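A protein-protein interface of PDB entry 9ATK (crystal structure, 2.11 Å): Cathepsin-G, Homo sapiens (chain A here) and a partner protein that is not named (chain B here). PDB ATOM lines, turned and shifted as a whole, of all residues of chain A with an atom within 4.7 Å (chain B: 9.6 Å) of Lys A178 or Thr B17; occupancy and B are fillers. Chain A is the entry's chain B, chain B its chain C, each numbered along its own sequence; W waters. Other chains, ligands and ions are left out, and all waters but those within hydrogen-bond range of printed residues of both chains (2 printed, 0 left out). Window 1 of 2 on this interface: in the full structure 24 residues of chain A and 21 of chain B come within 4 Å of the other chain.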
ATOM      1  N   HIS A  44      21.426  -6.368 -12.946  1.00  0.00           N
ATOM      2  CA  HIS A  44      21.782  -5.416 -13.989  1.00  0.00           C
ATOM      3  C   HIS A  44      21.978  -4.010 -13.441  1.00  0.00           C
ATOM      4  O   HIS A  44      22.339  -3.127 -14.216  1.00  0.00           O
ATOM      5  CB  HIS A  44      20.735  -5.429 -15.110  1.00  0.00           C
ATOM      6  CG  HIS A  44      19.434  -4.785 -14.744  1.00  0.00           C
ATOM      7  ND1 HIS A  44      18.320  -5.507 -14.370  1.00  0.00           N
ATOM      8  CD2 HIS A  44      19.053  -3.484 -14.747  1.00  0.00           C
ATOM      9  CE1 HIS A  44      17.319  -4.678 -14.132  1.00  0.00           C
ATOM     10  NE2 HIS A  44      17.736  -3.447 -14.365  1.00  0.00           N
ATOM     11  N   ILE A  85      19.327 -11.917 -19.681  1.00  0.00           N
ATOM     12  CA  ILE A  85      18.787 -11.341 -18.445  1.00  0.00           C
ATOM     13  C   ILE A  85      18.175 -12.434 -17.576  1.00  0.00           C
ATOM     14  O   ILE A  85      17.070 -12.279 -17.053  1.00  0.00           O
ATOM     15  CB  ILE A  85      17.746 -10.233 -18.705  1.00  0.00           C
ATOM     16  CG1 ILE A  85      18.090  -9.426 -19.965  1.00  0.00           C
ATOM     17  CG2 ILE A  85      17.654  -9.291 -17.490  1.00  0.00           C
ATOM     18  CD1 ILE A  85      17.127  -8.260 -20.206  1.00  0.00           C
ATOM     19  N   GLY A 128      11.239   5.807 -10.715  1.00  0.00           N
ATOM     20  CA  GLY A 128      11.503   5.886 -12.133  1.00  0.00           C
ATOM     21  C   GLY A 128      10.597   6.891 -12.822  1.00  0.00           C
ATOM     22  O   GLY A 128       9.703   7.508 -12.231  1.00  0.00           O
ATOM     23  N   ARG A 129      10.839   7.049 -14.119  1.00  0.00           N
ATOM     24  CA  ARG A 129      10.089   8.019 -14.908  1.00  0.00           C
ATOM     25  C   ARG A 129       8.613   7.618 -15.008  1.00  0.00           C
ATOM     26  O   ARG A 129       8.234   6.453 -14.829  1.00  0.00           O
ATOM     27  CB  ARG A 129      10.717   8.147 -16.288  1.00  0.00           C
ATOM     28  CG  ARG A 129      12.223   8.301 -16.225  1.00  0.00           C
ATOM     29  CD  ARG A 129      12.609   9.741 -16.053  1.00  0.00           C
ATOM     30  NE  ARG A 129      12.262  10.491 -17.258  1.00  0.00           N
ATOM     31  CZ  ARG A 129      12.414  11.802 -17.388  1.00  0.00           C
ATOM     32  NH1 ARG A 129      12.916  12.537 -16.409  1.00  0.00           N
ATOM     33  NH2 ARG A 129      12.051  12.389 -18.528  1.00  0.00           N
ATOM     34  N   PHE A 177       9.057   1.615 -15.210  1.00  0.00           N
ATOM     35  CA  PHE A 177       9.729   2.315 -16.291  1.00  0.00           C
ATOM     36  C   PHE A 177      11.105   2.753 -15.790  1.00  0.00           C
ATOM     37  O   PHE A 177      11.553   2.326 -14.723  1.00  0.00           O
ATOM     38  CB  PHE A 177       8.851   3.467 -16.801  1.00  0.00           C
ATOM     39  CG  PHE A 177       9.253   3.973 -18.148  1.00  0.00           C
ATOM     40  CD1 PHE A 177       9.492   3.084 -19.190  1.00  0.00           C
ATOM     41  CD2 PHE A 177       9.396   5.323 -18.382  1.00  0.00           C
ATOM     42  CE1 PHE A 177       9.870   3.545 -20.442  1.00  0.00           C
ATOM     43  CE2 PHE A 177       9.778   5.793 -19.621  1.00  0.00           C
ATOM     44  CZ  PHE A 177      10.021   4.904 -20.648  1.00  0.00           C
ATOM     45  N   LYS A 178      11.782   3.595 -16.573  1.00  0.00           N
ATOM     46  CA  LYS A 178      13.216   3.836 -16.405  1.00  0.00           C
ATOM     47  C   LYS A 178      13.532   4.398 -15.024  1.00  0.00           C
ATOM     48  O   LYS A 178      13.113   5.511 -14.681  1.00  0.00           O
ATOM     49  CB  LYS A 178      13.729   4.800 -17.486  1.00  0.00           C
ATOM     50  CG  LYS A 178      13.519   4.351 -18.943  1.00  0.00           C
ATOM     51  CD  LYS A 178      14.037   2.940 -19.185  1.00  0.00           C
ATOM     52  CE  LYS A 178      14.224   2.676 -20.692  1.00  0.00           C
ATOM     53  NZ  LYS A 178      14.682   1.277 -21.007  1.00  0.00           N
ATOM     54  N   GLY A 179      14.308   3.644 -14.254  1.00  0.00           N
ATOM     55  CA  GLY A 179      14.634   4.009 -12.887  1.00  0.00           C
ATOM     56  C   GLY A 179      13.978   3.122 -11.868  1.00  0.00           C
ATOM     57  O   GLY A 179      14.392   3.129 -10.706  1.00  0.00           O
ATOM     58  N   ASP A 180      12.967   2.351 -12.264  1.00  0.00           N
ATOM     59  CA  ASP A 180      12.339   1.416 -11.349  1.00  0.00           C
ATOM     60  C   ASP A 180      13.065   0.085 -11.242  1.00  0.00           C
ATOM     61  O   ASP A 180      12.708  -0.694 -10.356  1.00  0.00           O
ATOM     62  CB  ASP A 180      10.889   1.164 -11.776  1.00  0.00           C
ATOM     63  CG  ASP A 180      10.042   2.392 -11.613  1.00  0.00           C
ATOM     64  OD1 ASP A 180      10.278   3.098 -10.599  1.00  0.00           O
ATOM     65  OD2 ASP A 180       9.174   2.668 -12.495  1.00  0.00           O
ATOM     66  N   SER A 181      14.011  -0.213 -12.144  1.00  0.00           N
ATOM     67  CA  SER A 181      14.795  -1.451 -12.086  1.00  0.00           C
ATOM     68  C   SER A 181      15.172  -1.795 -10.649  1.00  0.00           C
ATOM     69  O   SER A 181      15.527  -0.913  -9.856  1.00  0.00           O
ATOM     70  CB  SER A 181      16.081  -1.294 -12.911  1.00  0.00           C
ATOM     71  OG  SER A 181      15.840  -1.453 -14.281  1.00  0.00           O
ATOM     72  N   SER A 196      12.819  -6.388 -13.498  1.00  0.00           N
ATOM     73  CA  SER A 196      13.920  -6.934 -14.290  1.00  0.00           C
ATOM     74  C   SER A 196      13.936  -6.411 -15.722  1.00  0.00           C
ATOM     75  O   SER A 196      14.873  -5.696 -16.089  1.00  0.00           O
ATOM     76  CB  SER A 196      13.891  -8.465 -14.270  1.00  0.00           C
ATOM     77  OG  SER A 196      15.063  -8.943 -14.920  1.00  0.00           O
ATOM     78  N   TYR A 197      12.990  -6.802 -16.573  1.00  0.00           N
ATOM     79  CA  TYR A 197      13.050  -6.285 -17.928  1.00  0.00           C
ATOM     80  C   TYR A 197      11.665  -6.314 -18.523  1.00  0.00           C
ATOM     81  O   TYR A 197      10.711  -6.832 -17.926  1.00  0.00           O
ATOM     82  CB  TYR A 197      14.043  -7.055 -18.814  1.00  0.00           C
ATOM     83  CG  TYR A 197      13.697  -8.504 -19.112  1.00  0.00           C
ATOM     84  CD1 TYR A 197      12.890  -8.852 -20.207  1.00  0.00           C
ATOM     85  CD2 TYR A 197      14.224  -9.530 -18.335  1.00  0.00           C
ATOM     86  CE1 TYR A 197      12.597 -10.204 -20.502  1.00  0.00           C
ATOM     87  CE2 TYR A 197      13.947 -10.885 -18.625  1.00  0.00           C
ATOM     88  CZ  TYR A 197      13.128 -11.209 -19.696  1.00  0.00           C
ATOM     89  OH  TYR A 197      12.881 -12.538 -19.943  1.00  0.00           O
ATOM     90  N   PRO B   7      22.232  10.605 -21.015  1.00  0.00           N
ATOM     91  CA  PRO B   7      21.253   9.508 -20.910  1.00  0.00           C
ATOM     92  C   PRO B   7      21.282   8.587 -22.134  1.00  0.00           C
ATOM     93  O   PRO B   7      21.357   9.044 -23.277  1.00  0.00           O
ATOM     94  CB  PRO B   7      19.912  10.247 -20.803  1.00  0.00           C
ATOM     95  CG  PRO B   7      20.267  11.667 -20.357  1.00  0.00           C
ATOM     96  CD  PRO B   7      21.590  11.936 -20.982  1.00  0.00           C
ATOM     97  N   TYR B   8      21.197   7.281 -21.893  1.00  0.00           N
ATOM     98  CA  TYR B   8      21.220   6.339 -22.998  1.00  0.00           C
ATOM     99  C   TYR B   8      20.425   5.088 -22.640  1.00  0.00           C
ATOM    100  O   TYR B   8      20.272   4.745 -21.469  1.00  0.00           O
ATOM    101  CB  TYR B   8      22.652   5.976 -23.382  1.00  0.00           C
ATOM    102  CG  TYR B   8      23.213   4.848 -22.573  1.00  0.00           C
ATOM    103  CD1 TYR B   8      23.724   5.065 -21.293  1.00  0.00           C
ATOM    104  CD2 TYR B   8      23.209   3.554 -23.077  1.00  0.00           C
ATOM    105  CE1 TYR B   8      24.226   4.014 -20.550  1.00  0.00           C
ATOM    106  CE2 TYR B   8      23.695   2.508 -22.354  1.00  0.00           C
ATOM    107  CZ  TYR B   8      24.197   2.732 -21.089  1.00  0.00           C
ATOM    108  OH  TYR B   8      24.685   1.659 -20.403  1.00  0.00           O
ATOM    109  N   THR B   9      19.919   4.402 -23.663  1.00  0.00           N
ATOM    110  CA  THR B   9      19.232   3.132 -23.466  1.00  0.00           C
ATOM    111  C   THR B   9      19.802   2.079 -24.412  1.00  0.00           C
ATOM    112  O   THR B   9      20.368   2.396 -25.467  1.00  0.00           O
ATOM    113  CB  THR B   9      17.714   3.274 -23.695  1.00  0.00           C
ATOM    114  OG1 THR B   9      17.466   3.603 -25.070  1.00  0.00           O
ATOM    115  CG2 THR B   9      17.124   4.382 -22.826  1.00  0.00           C
ATOM    116  N   ILE B  10      19.625   0.812 -24.042  1.00  0.00           N
ATOM    117  CA  ILE B  10      19.899  -0.318 -24.927  1.00  0.00           C
ATOM    118  C   ILE B  10      18.629  -1.131 -25.113  1.00  0.00           C
ATOM    119  O   ILE B  10      18.005  -1.539 -24.132  1.00  0.00           O
ATOM    120  CB  ILE B  10      20.996  -1.239 -24.377  1.00  0.00           C
ATOM    121  CG1 ILE B  10      22.319  -0.483 -24.240  1.00  0.00           C
ATOM    122  CG2 ILE B  10      21.108  -2.508 -25.268  1.00  0.00           C
ATOM    123  CD1 ILE B  10      23.365  -1.233 -23.465  1.00  0.00           C
ATOM    124  N   ALA B  11      18.303  -1.450 -26.357  1.00  0.00           N
ATOM    125  CA  ALA B  11      17.269  -2.425 -26.664  1.00  0.00           C
ATOM    126  C   ALA B  11      17.889  -3.555 -27.480  1.00  0.00           C
ATOM    127  O   ALA B  11      18.621  -3.298 -28.443  1.00  0.00           O
ATOM    128  CB  ALA B  11      16.104  -1.766 -27.408  1.00  0.00           C
ATOM    129  N   VAL B  12      17.623  -4.800 -27.076  1.00  0.00           N
ATOM    130  CA  VAL B  12      18.060  -5.993 -27.796  1.00  0.00           C
ATOM    131  C   VAL B  12      16.818  -6.791 -28.152  1.00  0.00           C
ATOM    132  O   VAL B  12      16.097  -7.249 -27.260  1.00  0.00           O
ATOM    133  CB  VAL B  12      19.032  -6.852 -26.978  1.00  0.00           C
ATOM    134  CG1 VAL B  12      19.511  -8.052 -27.824  1.00  0.00           C
ATOM    135  CG2 VAL B  12      20.206  -6.006 -26.473  1.00  0.00           C
ATOM    136  N   GLY B  14      14.120  -5.654 -29.106  1.00  0.00           N
ATOM    137  CA  GLY B  14      13.030  -4.965 -28.451  1.00  0.00           C
ATOM    138  C   GLY B  14      13.005  -5.022 -26.929  1.00  0.00           C
ATOM    139  O   GLY B  14      12.165  -4.351 -26.315  1.00  0.00           O
ATOM    140  N   THR B  15      13.882  -5.778 -26.285  1.00  0.00           N
ATOM    141  CA  THR B  15      13.844  -5.870 -24.835  1.00  0.00           C
ATOM    142  C   THR B  15      14.935  -5.022 -24.197  1.00  0.00           C
ATOM    143  O   THR B  15      16.067  -4.957 -24.685  1.00  0.00           O
ATOM    144  CB  THR B  15      13.974  -7.316 -24.352  1.00  0.00           C
ATOM    145  OG1 THR B  15      15.337  -7.759 -24.502  1.00  0.00           O
ATOM    146  CG2 THR B  15      13.019  -8.210 -25.132  1.00  0.00           C
ATOM    147  N   SER B  16      14.588  -4.405 -23.080  1.00  0.00           N
ATOM    148  CA  SER B  16      15.518  -3.597 -22.319  1.00  0.00           C
ATOM    149  C   SER B  16      15.190  -3.739 -20.840  1.00  0.00           C
ATOM    150  O   SER B  16      14.093  -4.160 -20.465  1.00  0.00           O
ATOM    151  CB  SER B  16      15.436  -2.128 -22.724  1.00  0.00           C
ATOM    152  OG  SER B  16      14.112  -1.696 -22.548  1.00  0.00           O
ATOM    153  N   THR B  17      16.171  -3.403 -20.007  1.00  0.00           N
ATOM    154  CA  THR B  17      16.001  -3.273 -18.584  1.00  0.00           C
ATOM    155  C   THR B  17      15.615  -1.836 -18.262  1.00  0.00           C
ATOM    156  O   THR B  17      16.205  -0.907 -18.814  1.00  0.00           O
ATOM    157  CB  THR B  17      17.296  -3.628 -17.848  1.00  0.00           C
ATOM    158  OG1 THR B  17      18.379  -2.862 -18.389  1.00  0.00           O
ATOM    159  CG2 THR B  17      17.612  -5.123 -17.964  1.00  0.00           C
ATOM    160  N   PRO B  18      14.600  -1.612 -17.415  1.00  0.00           N
ATOM    161  CA  PRO B  18      14.153  -0.234 -17.111  1.00  0.00           C
ATOM    162  C   PRO B  18      15.081   0.482 -16.130  1.00  0.00           C
ATOM    163  O   PRO B  18      14.707   0.840 -15.024  1.00  0.00           O
ATOM    164  CB  PRO B  18      12.755  -0.469 -16.524  1.00  0.00           C
ATOM    165  CG  PRO B  18      12.879  -1.805 -15.808  1.00  0.00           C
ATOM    166  CD  PRO B  18      13.833  -2.630 -16.672  1.00  0.00           C
ATOM    167  N   ILE B  19      16.321   0.686 -16.533  1.00  0.00           N
ATOM    168  CA  ILE B  19      17.315   1.362 -15.711  1.00  0.00           C
ATOM    169  C   ILE B  19      17.482   2.788 -16.230  1.00  0.00           C
ATOM    170  O   ILE B  19      17.377   3.032 -17.436  1.00  0.00           O
ATOM    171  CB  ILE B  19      18.645   0.577 -15.723  1.00  0.00           C
ATOM    172  CG1 ILE B  19      19.656   1.185 -14.740  1.00  0.00           C
ATOM    173  CG2 ILE B  19      19.213   0.474 -17.141  1.00  0.00           C
ATOM    174  CD1 ILE B  19      20.757   0.214 -14.283  1.00  0.00           C
ATOM    175  N   LEU B  20      17.686   3.745 -15.322  1.00  0.00           N
ATOM    176  CA  LEU B  20      18.016   5.112 -15.714  1.00  0.00           C
ATOM    177  C   LEU B  20      19.535   5.206 -15.827  1.00  0.00           C
ATOM    178  O   LEU B  20      20.237   5.209 -14.808  1.00  0.00           O
ATOM    179  CB  LEU B  20      17.491   6.119 -14.702  1.00  0.00           C
ATOM    180  CG  LEU B  20      16.319   7.018 -15.094  1.00  0.00           C
ATOM    181  CD1 LEU B  20      16.091   8.062 -14.006  1.00  0.00           C
ATOM    182  CD2 LEU B  20      16.471   7.669 -16.499  1.00  0.00           C
ATOM    183  N   SER B  21      20.052   5.279 -17.052  1.00  0.00           N
ATOM    184  CA  SER B  21      21.490   5.142 -17.273  1.00  0.00           C
ATOM    185  C   SER B  21      22.048   6.299 -18.091  1.00  0.00           C
ATOM    186  O   SER B  21      21.397   6.786 -19.024  1.00  0.00           O
ATOM    187  CB  SER B  21      21.815   3.814 -17.975  1.00  0.00           C
ATOM    188  OG  SER B  21      21.819   2.753 -17.030  1.00  0.00           O
ATOM    189  N   VAL B  43      29.413  -0.455 -23.715  1.00  0.00           N
ATOM    190  CA  VAL B  43      28.292  -0.757 -22.833  1.00  0.00           C
ATOM    191  C   VAL B  43      27.397  -1.854 -23.418  1.00  0.00           C
ATOM    192  O   VAL B  43      26.790  -2.612 -22.658  1.00  0.00           O
ATOM    193  CB  VAL B  43      27.496   0.517 -22.462  1.00  0.00           C
ATOM    194  CG1 VAL B  43      28.344   1.423 -21.533  1.00  0.00           C
ATOM    195  CG2 VAL B  43      27.068   1.271 -23.651  1.00  0.00           C
ATOM    196  N   GLU B  47      26.930  -4.285 -20.446  1.00  0.00           N
ATOM    197  CA  GLU B  47      25.595  -4.367 -19.858  1.00  0.00           C
ATOM    198  C   GLU B  47      24.718  -5.461 -20.463  1.00  0.00           C
ATOM    199  O   GLU B  47      23.884  -6.036 -19.737  1.00  0.00           O
ATOM    200  CB  GLU B  47      24.867  -3.023 -19.970  1.00  0.00           C
ATOM    201  CG  GLU B  47      25.539  -1.847 -19.265  1.00  0.00           C
ATOM    202  CD  GLU B  47      26.113  -2.182 -17.889  1.00  0.00           C
ATOM    203  OE1 GLU B  47      25.335  -2.323 -16.904  1.00  0.00           O
ATOM    204  OE2 GLU B  47      27.362  -2.288 -17.808  1.00  0.00           O
ATOM    205  N   ARG B  48      24.881  -5.796 -21.758  1.00  0.00           N
ATOM    206  CA  ARG B  48      23.995  -6.792 -22.372  1.00  0.00           C
ATOM    207  C   ARG B  48      24.710  -7.978 -23.015  1.00  0.00           C
ATOM    208  O   ARG B  48      24.059  -8.759 -23.728  1.00  0.00           O
ATOM    209  CB  ARG B  48      23.063  -6.137 -23.406  1.00  0.00           C
ATOM    210  CG  ARG B  48      21.953  -5.265 -22.784  1.00  0.00           C
ATOM    211  CD  ARG B  48      21.046  -6.037 -21.786  1.00  0.00           C
ATOM    212  NE  ARG B  48      20.422  -7.234 -22.362  1.00  0.00           N
ATOM    213  CZ  ARG B  48      19.260  -7.244 -23.009  1.00  0.00           C
ATOM    214  NH1 ARG B  48      18.530  -6.147 -23.133  1.00  0.00           N
ATOM    215  NH2 ARG B  48      18.828  -8.380 -23.566  1.00  0.00           N
ATOM    216  N   LYS B  94      20.350  12.672 -25.774  1.00  0.00           N
ATOM    217  CA  LYS B  94      20.292  11.274 -25.363  1.00  0.00           C
ATOM    218  C   LYS B  94      20.723  10.401 -26.539  1.00  0.00           C
ATOM    219  O   LYS B  94      20.811  10.857 -27.688  1.00  0.00           O
ATOM    220  CB  LYS B  94      18.890  10.878 -24.889  1.00  0.00           C
ATOM    221  CG  LYS B  94      17.843  10.907 -25.994  1.00  0.00           C
ATOM    222  CD  LYS B  94      16.765   9.871 -25.723  1.00  0.00           C
ATOM    223  CE  LYS B  94      15.893   9.618 -26.943  1.00  0.00           C
ATOM    224  NZ  LYS B  94      14.719  10.496 -26.959  1.00  0.00           N
ATOM    225  N   ILE B  95      20.976   9.126 -26.238  1.00  0.00           N
ATOM    226  CA  ILE B  95      21.429   8.150 -27.234  1.00  0.00           C
ATOM    227  C   ILE B  95      20.640   6.869 -27.012  1.00  0.00           C
ATOM    228  O   ILE B  95      20.681   6.304 -25.913  1.00  0.00           O
ATOM    229  CB  ILE B  95      22.939   7.851 -27.130  1.00  0.00           C
ATOM    230  CG1 ILE B  95      23.765   9.115 -27.368  1.00  0.00           C
ATOM    231  CG2 ILE B  95      23.355   6.725 -28.099  1.00  0.00           C
ATOM    232  CD1 ILE B  95      25.209   9.000 -26.845  1.00  0.00           C
ATOM    233  N   ASP B  96      19.918   6.413 -28.035  1.00  0.00           N
ATOM    234  CA  ASP B  96      19.180   5.157 -27.977  1.00  0.00           C
ATOM    235  C   ASP B  96      19.894   4.117 -28.834  1.00  0.00           C
ATOM    236  O   ASP B  96      20.015   4.294 -30.048  1.00  0.00           O
ATOM    237  CB  ASP B  96      17.742   5.341 -28.463  1.00  0.00           C
ATOM    238  CG  ASP B  96      16.892   6.156 -27.505  1.00  0.00           C
ATOM    239  OD1 ASP B  96      17.104   6.103 -26.264  1.00  0.00           O
ATOM    240  OD2 ASP B  96      15.979   6.834 -28.002  1.00  0.00           O
ATOM    241  N   ILE B  97      20.356   3.040 -28.202  1.00  0.00           N
ATOM    242  CA  ILE B  97      21.037   1.936 -28.870  1.00  0.00           C
ATOM    243  C   ILE B  97      20.041   0.823 -29.128  1.00  0.00           C
ATOM    244  O   ILE B  97      19.241   0.472 -28.241  1.00  0.00           O
ATOM    245  CB  ILE B  97      22.201   1.413 -28.012  1.00  0.00           C
ATOM    246  CG1 ILE B  97      23.101   2.573 -27.585  1.00  0.00           C
ATOM    247  CG2 ILE B  97      22.934   0.303 -28.750  1.00  0.00           C
ATOM    248  CD1 ILE B  97      23.884   2.291 -26.254  1.00  0.00           C
HETATM  249  O   HOH W   1      16.540   1.706 -12.765  1.00  0.00           O
HETATM  250  O   HOH W   2      17.262   2.626 -19.806  1.00  0.00           O
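The backbone carbonyl oxygen (O) of Phe A177 lies close to the backbone carbonyl oxygen (O) of Pro B18, at 3.5 Å. The side-chain amino group (NZ) of Lys A178 lies within hydrogen-bond range of the side-chain hydroxyl (OG) of Ser B16. The side-chain hydroxyl (OG) of Ser A181 sits at hydrogen-bond distance from the backbone NH (N) of Ile B19, 3.1 Å away. The backbone carbonyl oxygen (O) of Pro B18 sits at hydrogen-bond distance from the side-chain hydroxyl (OG) of Ser A181, at 2.7 Å. NZ of Lys A178 is in hydrogen-bond range of O of Thr B17, 3.4 Å away. The backbone carbonyl oxygen (O) of Pro B18 sits at hydrogen-bond distance from the backbone NH (N) of Gly A179.
O of Lys A178 sits at hydrogen-bond distance from N of Arg A129. O of Thr B15 sits at hydrogen-bond distance from NH1 of Arg B48. N of Phe A177 lies within hydrogen-bond range of OD2 of Asp A180, at 2.9 Å. OD1 of Asp A180 is in hydrogen-bond range of N of Gly A128 (2.9 Å). The backbone NH of Thr B9 is in hydrogen-bond range of the backbone carbonyl oxygen of Ile B95 (3.0 Å). The side-chain hydroxyl (OG1) of Thr B9 sits at hydrogen-bond distance from the side-chain carboxylate (OD1) of Asp B96 (2.8 Å).
Ile B19 touches His A44 (CD1 to O, 3.7 Å). Thr B17 touches Ile A85. Ile A85 touches Arg B48. Pro B18 touches Lys A178 (O to CA, 3.6 Å). Ile B19 touches Lys A178 (O to CD, 3.8 Å). CG of Leu B20 touches O of Lys A178, at 3.6 Å. N of Gly A179 touches N of Leu B20, at 3.5 Å. O of Pro B18 touches N of Asp A180 (3.6 Å). Ser B16 touches Tyr A197 (O to CB, 3.3 Å). Tyr A197 touches Pro B18 (CA to CD, 3.9 Å).
Of chain B, only Pro B18 comes within 4 Å of Phe A177. Printed residues of chain B within 4 Å of Lys A178: Thr B9 (3.98 Å), Ser B16 (3.4 Å), Thr B17 (3.4 Å), Pro B18 (3.6 Å), Ile B19 (3.8 Å) and Leu B20 (3.6 Å). Of the printed residues of chain B, Asp A180 touches Pro B18 (3.6 Å). Printed residues of chain B within 4 Å of Tyr A197: Ser B16 and Pro B18. Thr B15 touches none of the printed residues of chain A. Printed residues of chain A within 4 Å of Thr B17: His A44, Ile A85, Lys A178 and Ser A196. The nearest printed residue of chain A that does not touch Thr B17 is Ser A181 (4.01 Å). The nearest printed residue of chain B that does not touch Ile A85 is Thr B15 (4.7 Å).
Of the 21 printed residues of chain B, 7 touch a printed residue of chain A. Among the printed residues, 21 pairs touch across the chains.
Water W2 lies within hydrogen-bond range of O of Ile B19 and NZ of Lys A178. Water W1 lies within hydrogen-bond range of O of Pro B18 (3.0 Å), N of Ser A181 (3.2 Å), O of Gly A179 (3.3 Å) and N of Leu B20 (3.5 Å).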
